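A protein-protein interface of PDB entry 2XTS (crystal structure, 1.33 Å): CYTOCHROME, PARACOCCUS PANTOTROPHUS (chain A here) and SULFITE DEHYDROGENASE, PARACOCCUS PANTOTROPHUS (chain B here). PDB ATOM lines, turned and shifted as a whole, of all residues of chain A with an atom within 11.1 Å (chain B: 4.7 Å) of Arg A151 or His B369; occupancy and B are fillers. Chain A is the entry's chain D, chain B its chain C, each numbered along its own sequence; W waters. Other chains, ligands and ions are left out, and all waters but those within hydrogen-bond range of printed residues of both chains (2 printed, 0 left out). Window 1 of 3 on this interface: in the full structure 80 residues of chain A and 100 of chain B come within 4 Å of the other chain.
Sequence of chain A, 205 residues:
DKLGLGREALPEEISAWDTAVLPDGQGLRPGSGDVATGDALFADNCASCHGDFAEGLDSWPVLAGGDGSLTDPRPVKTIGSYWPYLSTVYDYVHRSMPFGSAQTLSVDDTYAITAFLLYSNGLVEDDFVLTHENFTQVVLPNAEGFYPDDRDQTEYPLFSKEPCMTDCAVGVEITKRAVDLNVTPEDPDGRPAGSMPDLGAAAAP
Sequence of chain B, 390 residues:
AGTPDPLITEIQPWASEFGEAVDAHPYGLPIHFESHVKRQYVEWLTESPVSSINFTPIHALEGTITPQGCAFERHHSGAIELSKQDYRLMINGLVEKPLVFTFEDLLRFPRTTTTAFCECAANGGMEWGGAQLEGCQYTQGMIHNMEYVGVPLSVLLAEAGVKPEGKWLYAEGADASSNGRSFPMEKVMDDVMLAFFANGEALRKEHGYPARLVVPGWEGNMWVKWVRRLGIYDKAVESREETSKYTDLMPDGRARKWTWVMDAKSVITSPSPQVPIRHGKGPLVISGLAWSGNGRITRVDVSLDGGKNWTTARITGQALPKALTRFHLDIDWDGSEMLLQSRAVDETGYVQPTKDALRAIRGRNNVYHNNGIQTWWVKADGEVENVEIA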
ATOM      1  N   TYR A  82     -13.062 -37.469 -25.258  1.00  0.00           N
ATOM      2  CA  TYR A  82     -11.679 -36.977 -25.247  1.00  0.00           C
ATOM      3  C   TYR A  82     -10.635 -37.836 -24.537  1.00  0.00           C
ATOM      4  O   TYR A  82      -9.488 -37.870 -24.979  1.00  0.00           O
ATOM      5  CB  TYR A  82     -11.633 -35.562 -24.690  1.00  0.00           C
ATOM      6  CG  TYR A  82     -10.315 -34.838 -24.827  1.00  0.00           C
ATOM      7  CD1 TYR A  82      -9.829 -34.486 -26.070  1.00  0.00           C
ATOM      8  CD2 TYR A  82      -9.594 -34.434 -23.717  1.00  0.00           C
ATOM      9  CE1 TYR A  82      -8.618 -33.800 -26.198  1.00  0.00           C
ATOM     10  CE2 TYR A  82      -8.417 -33.740 -23.837  1.00  0.00           C
ATOM     11  CZ  TYR A  82      -7.921 -33.427 -25.082  1.00  0.00           C
ATOM     12  OH  TYR A  82      -6.761 -32.696 -25.245  1.00  0.00           O
ATOM     13  N   TYR A 147      -0.728 -37.220 -29.530  1.00  0.00           N
ATOM     14  CA  TYR A 147       0.628 -37.520 -29.983  1.00  0.00           C
ATOM     15  C   TYR A 147       1.591 -36.665 -29.191  1.00  0.00           C
ATOM     16  O   TYR A 147       1.253 -35.552 -28.815  1.00  0.00           O
ATOM     17  CB  TYR A 147       0.773 -37.307 -31.492  1.00  0.00           C
ATOM     18  CG  TYR A 147       0.381 -35.926 -31.982  1.00  0.00           C
ATOM     19  CD1 TYR A 147      -0.921 -35.649 -32.355  1.00  0.00           C
ATOM     20  CD2 TYR A 147       1.314 -34.926 -32.148  1.00  0.00           C
ATOM     21  CE1 TYR A 147      -1.294 -34.413 -32.828  1.00  0.00           C
ATOM     22  CE2 TYR A 147       0.951 -33.668 -32.628  1.00  0.00           C
ATOM     23  CZ  TYR A 147      -0.345 -33.411 -32.965  1.00  0.00           C
ATOM     24  OH  TYR A 147      -0.661 -32.173 -33.458  1.00  0.00           O
ATOM     25  N   PRO A 148       2.811 -37.156 -28.955  1.00  0.00           N
ATOM     26  CA  PRO A 148       3.789 -36.378 -28.203  1.00  0.00           C
ATOM     27  C   PRO A 148       4.165 -35.078 -28.899  1.00  0.00           C
ATOM     28  O   PRO A 148       4.233 -34.991 -30.129  1.00  0.00           O
ATOM     29  CB  PRO A 148       5.002 -37.310 -28.070  1.00  0.00           C
ATOM     30  CG  PRO A 148       4.482 -38.629 -28.241  1.00  0.00           C
ATOM     31  CD  PRO A 148       3.317 -38.515 -29.198  1.00  0.00           C
ATOM     32  N   ASP A 149       4.433 -34.067 -28.082  1.00  0.00           N
ATOM     33  CA  ASP A 149       4.889 -32.743 -28.505  1.00  0.00           C
ATOM     34  C   ASP A 149       5.787 -32.830 -29.721  1.00  0.00           C
ATOM     35  O   ASP A 149       6.820 -33.469 -29.678  1.00  0.00           O
ATOM     36  CB  ASP A 149       5.693 -32.131 -27.351  1.00  0.00           C
ATOM     37  CG  ASP A 149       6.046 -30.675 -27.525  1.00  0.00           C
ATOM     38  OD1 ASP A 149       5.686 -30.023 -28.527  1.00  0.00           O
ATOM     39  OD2 ASP A 149       6.738 -30.178 -26.602  1.00  0.00           O
ATOM     40  N   ASP A 150       5.369 -32.165 -30.789  1.00  0.00           N
ATOM     41  CA  ASP A 150       6.129 -32.106 -32.037  1.00  0.00           C
ATOM     42  C   ASP A 150       6.459 -30.673 -32.423  1.00  0.00           C
ATOM     43  O   ASP A 150       6.684 -30.384 -33.590  1.00  0.00           O
ATOM     44  CB  ASP A 150       5.330 -32.798 -33.168  1.00  0.00           C
ATOM     45  CG  ASP A 150       4.064 -32.052 -33.546  1.00  0.00           C
ATOM     46  OD1 ASP A 150       3.606 -31.224 -32.732  1.00  0.00           O
ATOM     47  OD2 ASP A 150       3.502 -32.349 -34.635  1.00  0.00           O
ATOM     48  N   ARG A 151       6.481 -29.752 -31.460  1.00  0.00           N
ATOM     49  CA  ARG A 151       6.859 -28.362 -31.772  1.00  0.00           C
ATOM     50  C   ARG A 151       8.239 -28.277 -32.408  1.00  0.00           C
ATOM     51  O   ARG A 151       8.478 -27.429 -33.265  1.00  0.00           O
ATOM     52  CB  ARG A 151       6.801 -27.474 -30.529  1.00  0.00           C
ATOM     53  CG  ARG A 151       5.417 -27.150 -30.086  1.00  0.00           C
ATOM     54  CD  ARG A 151       5.426 -26.377 -28.779  1.00  0.00           C
ATOM     55  NE  ARG A 151       5.729 -27.231 -27.625  1.00  0.00           N
ATOM     56  CZ  ARG A 151       5.922 -26.800 -26.383  1.00  0.00           C
ATOM     57  NH1 ARG A 151       5.881 -25.507 -26.107  1.00  0.00           N
ATOM     58  NH2 ARG A 151       6.095 -27.679 -25.402  1.00  0.00           N
ATOM     59  N   ASP A 152       9.135 -29.185 -32.026  1.00  0.00           N
ATOM     60  CA  ASP A 152      10.466 -29.223 -32.622  1.00  0.00           C
ATOM     61  C   ASP A 152      10.456 -29.447 -34.138  1.00  0.00           C
ATOM     62  O   ASP A 152      11.412 -29.078 -34.821  1.00  0.00           O
ATOM     63  CB  ASP A 152      11.359 -30.265 -31.925  1.00  0.00           C
ATOM     64  CG  ASP A 152      10.884 -31.703 -32.093  1.00  0.00           C
ATOM     65  OD1 ASP A 152       9.772 -31.974 -32.582  1.00  0.00           O
ATOM     66  OD2 ASP A 152      11.653 -32.601 -31.687  1.00  0.00           O
ATOM     67  N   GLN A 153       9.397 -30.056 -34.662  1.00  0.00           N
ATOM     68  CA  GLN A 153       9.246 -30.277 -36.103  1.00  0.00           C
ATOM     69  C   GLN A 153       8.361 -29.238 -36.769  1.00  0.00           C
ATOM     70  O   GLN A 153       8.645 -28.797 -37.884  1.00  0.00           O
ATOM     71  CB  GLN A 153       8.658 -31.662 -36.366  1.00  0.00           C
ATOM     72  CG  GLN A 153       9.535 -32.792 -35.879  1.00  0.00           C
ATOM     73  CD  GLN A 153       9.098 -34.144 -36.411  1.00  0.00           C
ATOM     74  OE1 GLN A 153       8.034 -34.664 -36.051  1.00  0.00           O
ATOM     75  NE2 GLN A 153       9.924 -34.726 -37.269  1.00  0.00           N
ATOM     76  N   THR A 154       7.301 -28.819 -36.080  1.00  0.00           N
ATOM     77  CA  THR A 154       6.222 -28.038 -36.661  1.00  0.00           C
ATOM     78  C   THR A 154       6.247 -26.538 -36.352  1.00  0.00           C
ATOM     79  O   THR A 154       5.552 -25.770 -37.019  1.00  0.00           O
ATOM     80  CB  THR A 154       4.856 -28.579 -36.238  1.00  0.00           C
ATOM     81  OG1 THR A 154       4.756 -28.523 -34.818  1.00  0.00           O
ATOM     82  CG2 THR A 154       4.659 -30.015 -36.719  1.00  0.00           C
ATOM     83  N   GLU A 155       7.012 -26.103 -35.340  1.00  0.00           N
ATOM     84  CA  GLU A 155       7.055 -24.701 -34.943  1.00  0.00           C
ATOM     85  C   GLU A 155       8.466 -24.153 -34.830  1.00  0.00           C
ATOM     86  O   GLU A 155       8.752 -23.061 -35.331  1.00  0.00           O
ATOM     87  CB  GLU A 155       6.319 -24.525 -33.607  1.00  0.00           C
ATOM     88  CG  GLU A 155       4.836 -24.854 -33.717  1.00  0.00           C
ATOM     89  CD  GLU A 155       4.021 -24.530 -32.473  1.00  0.00           C
ATOM     90  OE1 GLU A 155       4.510 -23.774 -31.604  1.00  0.00           O
ATOM     91  OE2 GLU A 155       2.876 -25.045 -32.405  1.00  0.00           O
ATOM     92  N   TYR A 156       9.371 -24.896 -34.202  1.00  0.00           N
ATOM     93  CA  TYR A 156      10.685 -24.327 -33.925  1.00  0.00           C
ATOM     94  C   TYR A 156      11.436 -23.951 -35.223  1.00  0.00           C
ATOM     95  O   TYR A 156      12.005 -22.875 -35.287  1.00  0.00           O
ATOM     96  CB  TYR A 156      11.500 -25.243 -33.020  1.00  0.00           C
ATOM     97  CG  TYR A 156      10.949 -25.455 -31.605  1.00  0.00           C
ATOM     98  CD1 TYR A 156       9.894 -24.705 -31.105  1.00  0.00           C
ATOM     99  CD2 TYR A 156      11.525 -26.398 -30.764  1.00  0.00           C
ATOM    100  CE1 TYR A 156       9.421 -24.906 -29.794  1.00  0.00           C
ATOM    101  CE2 TYR A 156      11.049 -26.614 -29.481  1.00  0.00           C
ATOM    102  CZ  TYR A 156      10.009 -25.849 -29.005  1.00  0.00           C
ATOM    103  OH  TYR A 156       9.542 -26.074 -27.733  1.00  0.00           O
ATOM    104  N   PRO A 157      11.386 -24.796 -36.273  1.00  0.00           N
ATOM    105  CA  PRO A 157      12.109 -24.343 -37.478  1.00  0.00           C
ATOM    106  C   PRO A 157      11.546 -23.047 -38.064  1.00  0.00           C
ATOM    107  O   PRO A 157      12.304 -22.125 -38.401  1.00  0.00           O
ATOM    108  CB  PRO A 157      11.955 -25.535 -38.424  1.00  0.00           C
ATOM    109  CG  PRO A 157      11.756 -26.731 -37.503  1.00  0.00           C
ATOM    110  CD  PRO A 157      10.877 -26.180 -36.411  1.00  0.00           C
ATOM    111  N   LEU A 158      10.229 -22.930 -38.120  1.00  0.00           N
ATOM    112  CA  LEU A 158       9.595 -21.735 -38.636  1.00  0.00           C
ATOM    113  C   LEU A 158       9.888 -20.495 -37.797  1.00  0.00           C
ATOM    114  O   LEU A 158      10.177 -19.416 -38.324  1.00  0.00           O
ATOM    115  CB  LEU A 158       8.086 -21.943 -38.721  1.00  0.00           C
ATOM    116  CG  LEU A 158       7.269 -20.834 -39.376  1.00  0.00           C
ATOM    117  CD1 LEU A 158       7.776 -20.494 -40.786  1.00  0.00           C
ATOM    118  CD2 LEU A 158       5.792 -21.244 -39.393  1.00  0.00           C
ATOM    119  N   PHE A 159       9.807 -20.641 -36.469  1.00  0.00           N
ATOM    120  CA  PHE A 159       9.941 -19.506 -35.565  1.00  0.00           C
ATOM    121  C   PHE A 159      11.399 -19.159 -35.292  1.00  0.00           C
ATOM    122  O   PHE A 159      11.681 -18.146 -34.676  1.00  0.00           O
ATOM    123  CB  PHE A 159       9.185 -19.771 -34.241  1.00  0.00           C
ATOM    124  CG  PHE A 159       7.688 -19.983 -34.406  1.00  0.00           C
ATOM    125  CD1 PHE A 159       6.992 -19.496 -35.508  1.00  0.00           C
ATOM    126  CD2 PHE A 159       6.959 -20.595 -33.403  1.00  0.00           C
ATOM    127  CE1 PHE A 159       5.638 -19.700 -35.633  1.00  0.00           C
ATOM    128  CE2 PHE A 159       5.585 -20.776 -33.522  1.00  0.00           C
ATOM    129  CZ  PHE A 159       4.938 -20.343 -34.644  1.00  0.00           C
ATOM    130  N   SER A 160      12.328 -19.982 -35.774  1.00  0.00           N
ATOM    131  CA  SER A 160      13.760 -19.682 -35.648  1.00  0.00           C
ATOM    132  C   SER A 160      14.348 -19.069 -36.920  1.00  0.00           C
ATOM    133  O   SER A 160      15.565 -18.908 -37.008  1.00  0.00           O
ATOM    134  CB  SER A 160      14.536 -20.927 -35.263  1.00  0.00           C
ATOM    135  OG  SER A 160      14.003 -21.488 -34.092  1.00  0.00           O
ATOM    136  N   LYS A 161      13.493 -18.717 -37.881  1.00  0.00           N
ATOM    137  CA  LYS A 161      13.953 -17.985 -39.068  1.00  0.00           C
ATOM    138  C   LYS A 161      14.334 -16.555 -38.656  1.00  0.00           C
ATOM    139  O   LYS A 161      13.838 -16.015 -37.655  1.00  0.00           O
ATOM    140  CB  LYS A 161      12.884 -17.994 -40.178  1.00  0.00           C
ATOM    141  CG  LYS A 161      12.637 -19.358 -40.785  1.00  0.00           C
ATOM    142  CD  LYS A 161      13.912 -20.001 -41.306  1.00  0.00           C
ATOM    143  CE  LYS A 161      13.627 -21.122 -42.296  1.00  0.00           C
ATOM    144  NZ  LYS A 161      12.375 -21.870 -41.979  1.00  0.00           N
ATOM    145  N   ALA B 121       1.047 -23.443 -17.390  1.00  0.00           N
ATOM    146  CA  ALA B 121       0.787 -23.754 -18.785  1.00  0.00           C
ATOM    147  C   ALA B 121      -0.335 -22.907 -19.369  1.00  0.00           C
ATOM    148  O   ALA B 121      -0.336 -22.612 -20.554  1.00  0.00           O
ATOM    149  CB  ALA B 121       0.431 -25.234 -18.908  1.00  0.00           C
ATOM    150  N   TRP B 128      -6.287 -16.763 -26.055  1.00  0.00           N
ATOM    151  CA  TRP B 128      -6.091 -17.500 -27.294  1.00  0.00           C
ATOM    152  C   TRP B 128      -7.053 -17.035 -28.369  1.00  0.00           C
ATOM    153  O   TRP B 128      -6.675 -17.012 -29.538  1.00  0.00           O
ATOM    154  CB  TRP B 128      -6.291 -18.992 -27.067  1.00  0.00           C
ATOM    155  CG  TRP B 128      -5.035 -19.771 -26.868  1.00  0.00           C
ATOM    156  CD1 TRP B 128      -4.742 -20.585 -25.808  1.00  0.00           C
ATOM    157  CD2 TRP B 128      -3.939 -19.892 -27.779  1.00  0.00           C
ATOM    158  NE1 TRP B 128      -3.525 -21.183 -25.987  1.00  0.00           N
ATOM    159  CE2 TRP B 128      -3.010 -20.779 -27.189  1.00  0.00           C
ATOM    160  CE3 TRP B 128      -3.636 -19.334 -29.026  1.00  0.00           C
ATOM    161  CZ2 TRP B 128      -1.806 -21.115 -27.795  1.00  0.00           C
ATOM    162  CZ3 TRP B 128      -2.428 -19.668 -29.619  1.00  0.00           C
ATOM    163  CH2 TRP B 128      -1.529 -20.555 -29.009  1.00  0.00           C
ATOM    164  N   GLU B 219       6.400 -26.636 -17.822  1.00  0.00           N
ATOM    165  CA  GLU B 219       5.134 -26.057 -17.418  1.00  0.00           C
ATOM    166  C   GLU B 219       4.866 -26.221 -15.943  1.00  0.00           C
ATOM    167  O   GLU B 219       5.190 -27.244 -15.329  1.00  0.00           O
ATOM    168  CB  GLU B 219       4.003 -26.653 -18.273  1.00  0.00           C
ATOM    169  CG  GLU B 219       3.700 -28.132 -18.029  1.00  0.00           C
ATOM    170  CD  GLU B 219       2.827 -28.785 -19.079  1.00  0.00           C
ATOM    171  OE1 GLU B 219       2.385 -28.103 -20.041  1.00  0.00           O
ATOM    172  OE2 GLU B 219       2.585 -30.004 -18.921  1.00  0.00           O
ATOM    173  N   ASP B 248      -3.154 -30.432 -25.564  1.00  0.00           N
ATOM    174  CA  ASP B 248      -3.319 -29.198 -26.338  1.00  0.00           C
ATOM    175  C   ASP B 248      -4.022 -29.543 -27.672  1.00  0.00           C
ATOM    176  O   ASP B 248      -3.401 -30.059 -28.619  1.00  0.00           O
ATOM    177  CB  ASP B 248      -1.944 -28.547 -26.625  1.00  0.00           C
ATOM    178  CG  ASP B 248      -1.038 -28.457 -25.424  1.00  0.00           C
ATOM    179  OD1 ASP B 248      -1.524 -28.517 -24.266  1.00  0.00           O
ATOM    180  OD2 ASP B 248       0.184 -28.361 -25.647  1.00  0.00           O
ATOM    181  N   ARG B 256      -1.872 -32.534 -28.857  1.00  0.00           N
ATOM    182  CA  ARG B 256      -0.533 -32.812 -28.367  1.00  0.00           C
ATOM    183  C   ARG B 256      -0.586 -33.193 -26.898  1.00  0.00           C
ATOM    184  O   ARG B 256      -1.298 -32.566 -26.119  1.00  0.00           O
ATOM    185  CB  ARG B 256       0.352 -31.580 -28.514  1.00  0.00           C
ATOM    186  CG  ARG B 256       0.680 -31.178 -29.926  1.00  0.00           C
ATOM    187  CD  ARG B 256       1.308 -29.824 -29.908  1.00  0.00           C
ATOM    188  NE  ARG B 256       1.776 -29.404 -31.211  1.00  0.00           N
ATOM    189  CZ  ARG B 256       2.082 -28.158 -31.519  1.00  0.00           C
ATOM    190  NH1 ARG B 256       1.921 -27.191 -30.643  1.00  0.00           N
ATOM    191  NH2 ARG B 256       2.526 -27.860 -32.727  1.00  0.00           N
ATOM    192  N   THR B 259       3.511 -31.704 -23.714  1.00  0.00           N
ATOM    193  CA  THR B 259       4.091 -30.433 -24.103  1.00  0.00           C
ATOM    194  C   THR B 259       4.676 -29.845 -22.832  1.00  0.00           C
ATOM    195  O   THR B 259       4.069 -29.031 -22.133  1.00  0.00           O
ATOM    196  CB  THR B 259       3.077 -29.536 -24.779  1.00  0.00           C
ATOM    197  OG1 THR B 259       1.876 -29.440 -23.985  1.00  0.00           O
ATOM    198  CG2 THR B 259       2.758 -30.091 -26.164  1.00  0.00           C
ATOM    199  N   TRP B 260       5.891 -30.262 -22.537  1.00  0.00           N
ATOM    200  CA  TRP B 260       6.484 -29.961 -21.276  1.00  0.00           C
ATOM    201  C   TRP B 260       7.135 -28.580 -21.287  1.00  0.00           C
ATOM    202  O   TRP B 260       6.970 -27.788 -20.343  1.00  0.00           O
ATOM    203  CB  TRP B 260       7.516 -31.026 -20.922  1.00  0.00           C
ATOM    204  CG  TRP B 260       6.943 -32.414 -20.774  1.00  0.00           C
ATOM    205  CD1 TRP B 260       5.803 -32.783 -20.122  1.00  0.00           C
ATOM    206  CD2 TRP B 260       7.527 -33.631 -21.265  1.00  0.00           C
ATOM    207  NE1 TRP B 260       5.659 -34.138 -20.179  1.00  0.00           N
ATOM    208  CE2 TRP B 260       6.699 -34.683 -20.878  1.00  0.00           C
ATOM    209  CE3 TRP B 260       8.677 -33.928 -21.993  1.00  0.00           C
ATOM    210  CZ2 TRP B 260       6.985 -36.008 -21.193  1.00  0.00           C
ATOM    211  CZ3 TRP B 260       8.937 -35.253 -22.325  1.00  0.00           C
ATOM    212  CH2 TRP B 260       8.103 -36.261 -21.917  1.00  0.00           C
ATOM    213  N   VAL B 261       7.927 -28.255 -22.314  1.00  0.00           N
ATOM    214  CA  VAL B 261       8.680 -27.005 -22.300  1.00  0.00           C
ATOM    215  C   VAL B 261       7.800 -25.796 -22.572  1.00  0.00           C
ATOM    216  O   VAL B 261       6.859 -25.849 -23.362  1.00  0.00           O
ATOM    217  CB  VAL B 261       9.909 -27.030 -23.237  1.00  0.00           C
ATOM    218  CG1 VAL B 261      10.864 -28.085 -22.818  1.00  0.00           C
ATOM    219  CG2 VAL B 261       9.516 -27.190 -24.679  1.00  0.00           C
ATOM    220  N   MET B 262       8.128 -24.710 -21.893  1.00  0.00           N
ATOM    221  CA  MET B 262       7.545 -23.394 -22.095  1.00  0.00           C
ATOM    222  C   MET B 262       8.458 -22.606 -23.044  1.00  0.00           C
ATOM    223  O   MET B 262       9.638 -22.422 -22.771  1.00  0.00           O
ATOM    224  CB  MET B 262       7.417 -22.677 -20.761  1.00  0.00           C
ATOM    225  CG  MET B 262       6.561 -23.426 -19.746  1.00  0.00           C
ATOM    226  SD  MET B 262       4.861 -23.734 -20.279  1.00  0.00           S
ATOM    227  CE  MET B 262       4.149 -22.104 -20.106  1.00  0.00           C
ATOM    228  N   ASP B 263       7.911 -22.141 -24.159  1.00  0.00           N
ATOM    229  CA  ASP B 263       8.689 -21.486 -25.181  1.00  0.00           C
ATOM    230  C   ASP B 263       8.944 -19.999 -24.879  1.00  0.00           C
ATOM    231  O   ASP B 263       8.314 -19.389 -24.024  1.00  0.00           O
ATOM    232  CB  ASP B 263       7.973 -21.619 -26.528  1.00  0.00           C
ATOM    233  CG  ASP B 263       7.860 -23.045 -27.011  1.00  0.00           C
ATOM    234  OD1 ASP B 263       8.779 -23.849 -26.732  1.00  0.00           O
ATOM    235  OD2 ASP B 263       6.850 -23.330 -27.702  1.00  0.00           O
ATOM    236  N   ARG B 362      -1.989 -23.896 -34.777  1.00  0.00           N
ATOM    237  CA  ARG B 362      -2.665 -24.585 -33.690  1.00  0.00           C
ATOM    238  C   ARG B 362      -4.167 -24.383 -33.624  1.00  0.00           C
ATOM    239  O   ARG B 362      -4.854 -25.087 -32.884  1.00  0.00           O
ATOM    240  CB  ARG B 362      -2.116 -24.100 -32.354  1.00  0.00           C
ATOM    241  CG  ARG B 362      -0.653 -24.325 -32.160  1.00  0.00           C
ATOM    242  CD  ARG B 362      -0.261 -23.838 -30.844  1.00  0.00           C
ATOM    243  NE  ARG B 362       1.147 -23.875 -30.573  1.00  0.00           N
ATOM    244  CZ  ARG B 362       1.657 -23.490 -29.421  1.00  0.00           C
ATOM    245  NH1 ARG B 362       0.851 -23.201 -28.391  1.00  0.00           N
ATOM    246  NH2 ARG B 362       2.962 -23.467 -29.270  1.00  0.00           N
ATOM    247  N   VAL B 367      -5.701 -24.013 -25.531  1.00  0.00           N
ATOM    248  CA  VAL B 367      -5.852 -23.749 -24.089  1.00  0.00           C
ATOM    249  C   VAL B 367      -4.539 -23.298 -23.436  1.00  0.00           C
ATOM    250  O   VAL B 367      -4.521 -22.318 -22.700  1.00  0.00           O
ATOM    251  CB  VAL B 367      -6.522 -24.908 -23.289  1.00  0.00           C
ATOM    252  CG1 VAL B 367      -6.635 -24.580 -21.803  1.00  0.00           C
ATOM    253  CG2 VAL B 367      -7.908 -25.232 -23.858  1.00  0.00           C
ATOM    254  N   TYR B 368      -3.459 -24.018 -23.706  1.00  0.00           N
ATOM    255  CA  TYR B 368      -2.193 -23.842 -23.022  1.00  0.00           C
ATOM    256  C   TYR B 368      -1.154 -23.256 -23.990  1.00  0.00           C
ATOM    257  O   TYR B 368      -1.366 -23.155 -25.206  1.00  0.00           O
ATOM    258  CB  TYR B 368      -1.732 -25.214 -22.528  1.00  0.00           C
ATOM    259  CG  TYR B 368      -2.738 -25.906 -21.640  1.00  0.00           C
ATOM    260  CD1 TYR B 368      -2.999 -25.449 -20.366  1.00  0.00           C
ATOM    261  CD2 TYR B 368      -3.450 -27.018 -22.089  1.00  0.00           C
ATOM    262  CE1 TYR B 368      -3.909 -26.087 -19.552  1.00  0.00           C
ATOM    263  CE2 TYR B 368      -4.372 -27.639 -21.265  1.00  0.00           C
ATOM    264  CZ  TYR B 368      -4.619 -27.172 -20.007  1.00  0.00           C
ATOM    265  OH  TYR B 368      -5.510 -27.852 -19.197  1.00  0.00           O
ATOM    266  N   HIS B 369       0.005 -22.925 -23.436  1.00  0.00           N
ATOM    267  CA  HIS B 369       1.163 -22.567 -24.222  1.00  0.00           C
ATOM    268  C   HIS B 369       0.956 -21.363 -25.149  1.00  0.00           C
ATOM    269  O   HIS B 369       1.480 -21.333 -26.260  1.00  0.00           O
ATOM    270  CB  HIS B 369       1.722 -23.783 -24.982  1.00  0.00           C
ATOM    271  CG  HIS B 369       2.196 -24.876 -24.078  1.00  0.00           C
ATOM    272  ND1 HIS B 369       3.390 -24.811 -23.400  1.00  0.00           N
ATOM    273  CD2 HIS B 369       1.616 -26.039 -23.704  1.00  0.00           C
ATOM    274  CE1 HIS B 369       3.515 -25.887 -22.637  1.00  0.00           C
ATOM    275  NE2 HIS B 369       2.458 -26.651 -22.809  1.00  0.00           N
ATOM    276  N   ASN B 370       0.242 -20.349 -24.699  1.00  0.00           N
ATOM    277  CA  ASN B 370       0.133 -19.112 -25.467  1.00  0.00           C
ATOM    278  C   ASN B 370       1.300 -18.186 -25.190  1.00  0.00           C
ATOM    279  O   ASN B 370       1.264 -17.411 -24.236  1.00  0.00           O
ATOM    280  CB  ASN B 370      -1.175 -18.402 -25.159  1.00  0.00           C
ATOM    281  CG  ASN B 370      -1.382 -17.164 -26.033  1.00  0.00           C
ATOM    282  OD1 ASN B 370      -0.541 -16.829 -26.888  1.00  0.00           O
ATOM    283  ND2 ASN B 370      -2.479 -16.452 -25.798  1.00  0.00           N
ATOM    284  N   ASN B 371       2.329 -18.258 -26.033  1.00  0.00           N
ATOM    285  CA  ASN B 371       3.449 -17.337 -25.924  1.00  0.00           C
ATOM    286  C   ASN B 371       3.423 -16.241 -26.965  1.00  0.00           C
ATOM    287  O   ASN B 371       4.461 -15.654 -27.274  1.00  0.00           O
ATOM    288  CB  ASN B 371       4.799 -18.057 -25.923  1.00  0.00           C
ATOM    289  CG  ASN B 371       5.078 -18.819 -27.197  1.00  0.00           C
ATOM    290  OD1 ASN B 371       4.195 -19.445 -27.763  1.00  0.00           O
ATOM    291  ND2 ASN B 371       6.344 -18.793 -27.631  1.00  0.00           N
HETATM  292  O   HOH W   1       8.243 -30.495 -24.293  1.00  0.00           O
HETATM  293  O   HOH W   2       6.697 -22.688 -30.424  1.00  0.00           O
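Among the printed residues, pairs that only touch across the chains: Tyr A147 with Arg B256, Asp A149 with Thr B259, Arg A151 with Arg B256, Arg A151 with Thr B259, Arg A151 with Trp B260, Arg A151 with Arg B362, Arg A151 with His B369 and Tyr A156 with Val B261.
Of the 16 printed residues of chain A, 7 touch a printed residue of chain B. Hydrophobic or aromatic side chains of chain B within 4 Å of the printed part of chain A: Val B261 and His B369. Among the printed residues, Asp or Glu carboxylates within 4 Å of a Lys or Arg side-chain nitrogen of the other chain: Asp A150 with Arg B256, Arg A151 with Asp B263, Glu A155 with Arg B256 and Glu A155 with Arg B362.
O of Ala B121 sits at hydrogen-bond distance from N of His B369 (2.9 Å). The backbone carbonyl oxygen (O) of Trp B260 is in hydrogen-bond range of the backbone NH (N) of Glu B219 (2.8 Å). OD2 of Asp B248 lies close to OG1 of Thr B259. ND1 of His B369 lies close to SD of Met B262, 3.6 Å away. The guanidinium group (NH1) of Arg B362 is in hydrogen-bond range of the backbone carbonyl oxygen (O) of His B369, 2.9 Å away. OG of Ser A160 is in hydrogen-bond range of O of Tyr A156 (2.7 Å).
Pro A148 touches none of the printed residues of chain B. Printed residues of chain B within 4 Å of Arg A151: Arg B256 (3.5 Å), Thr B259 (3.6 Å), Trp B260 (3.9 Å), Val B261 (2.8 Å), Asp B263 (2.9 Å), Arg B362 (3.8 Å) and His B369 (3.7 Å). Printed residues of chain B within 4 Å of Glu A155: Arg B256 (2.9 Å) and Arg B362 (2.8 Å). Printed residues of chain B within 4 Å of Tyr A156: Val B261 and Asp B263. No residue of chain A comes within 4 Å of Ala B121. Of the printed residues of chain A, Arg B256 touches Tyr A147, Asp A150, Arg A151, Thr A154 and Glu A155. No residue of chain A comes within 4 Å of Met B262. Asp B263 touches just these residues of chain A: Arg A151 (2.9 Å) and Tyr A156 (2.6 Å). Of the printed residues of chain A, Arg B362 touches Arg A151 and Glu A155. His B369 touches just one residue of chain A: Arg A151 (3.7 Å).
Water W2 lies within hydrogen-bond range of the side-chain carboxylate (OE1) of Glu A155 (2.7 Å) and the side-chain carboxylate (OD2) of Asp B263 (2.8 Å). Water W1 lies within hydrogen-bond range of OD2 of Asp A149 (2.8 Å), N of Trp B260 (2.9 Å) and N of Val B261 (3.0 Å).
The guanidinium group of Arg B256 lies within salt-bridge range of the side-chain carboxylate of Asp A150 (3.0 Å). The side-chain hydroxyl (OG1) of Thr A154 lies within hydrogen-bond range of the guanidinium group (NH2) of Arg B256 (3.1 Å). NH2 of Arg B256 is in salt-bridge range of OE2 of Glu A155, 2.9 Å away. The backbone carbonyl oxygen of Val B261 is in hydrogen-bond range of the guanidinium group of Arg A151, 2.8 Å away. The side-chain carboxylate (OD2) of Asp B263 is in salt-bridge range of the guanidinium group (NH1) of Arg A151, at 2.9 Å. OD1 of Asp B263 is in hydrogen-bond range of OH of Tyr A156, 2.6 Å away. The side-chain carboxylate (OE2) of Glu A155 is in salt-bridge range of the guanidinium group (NE) of Arg B362.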
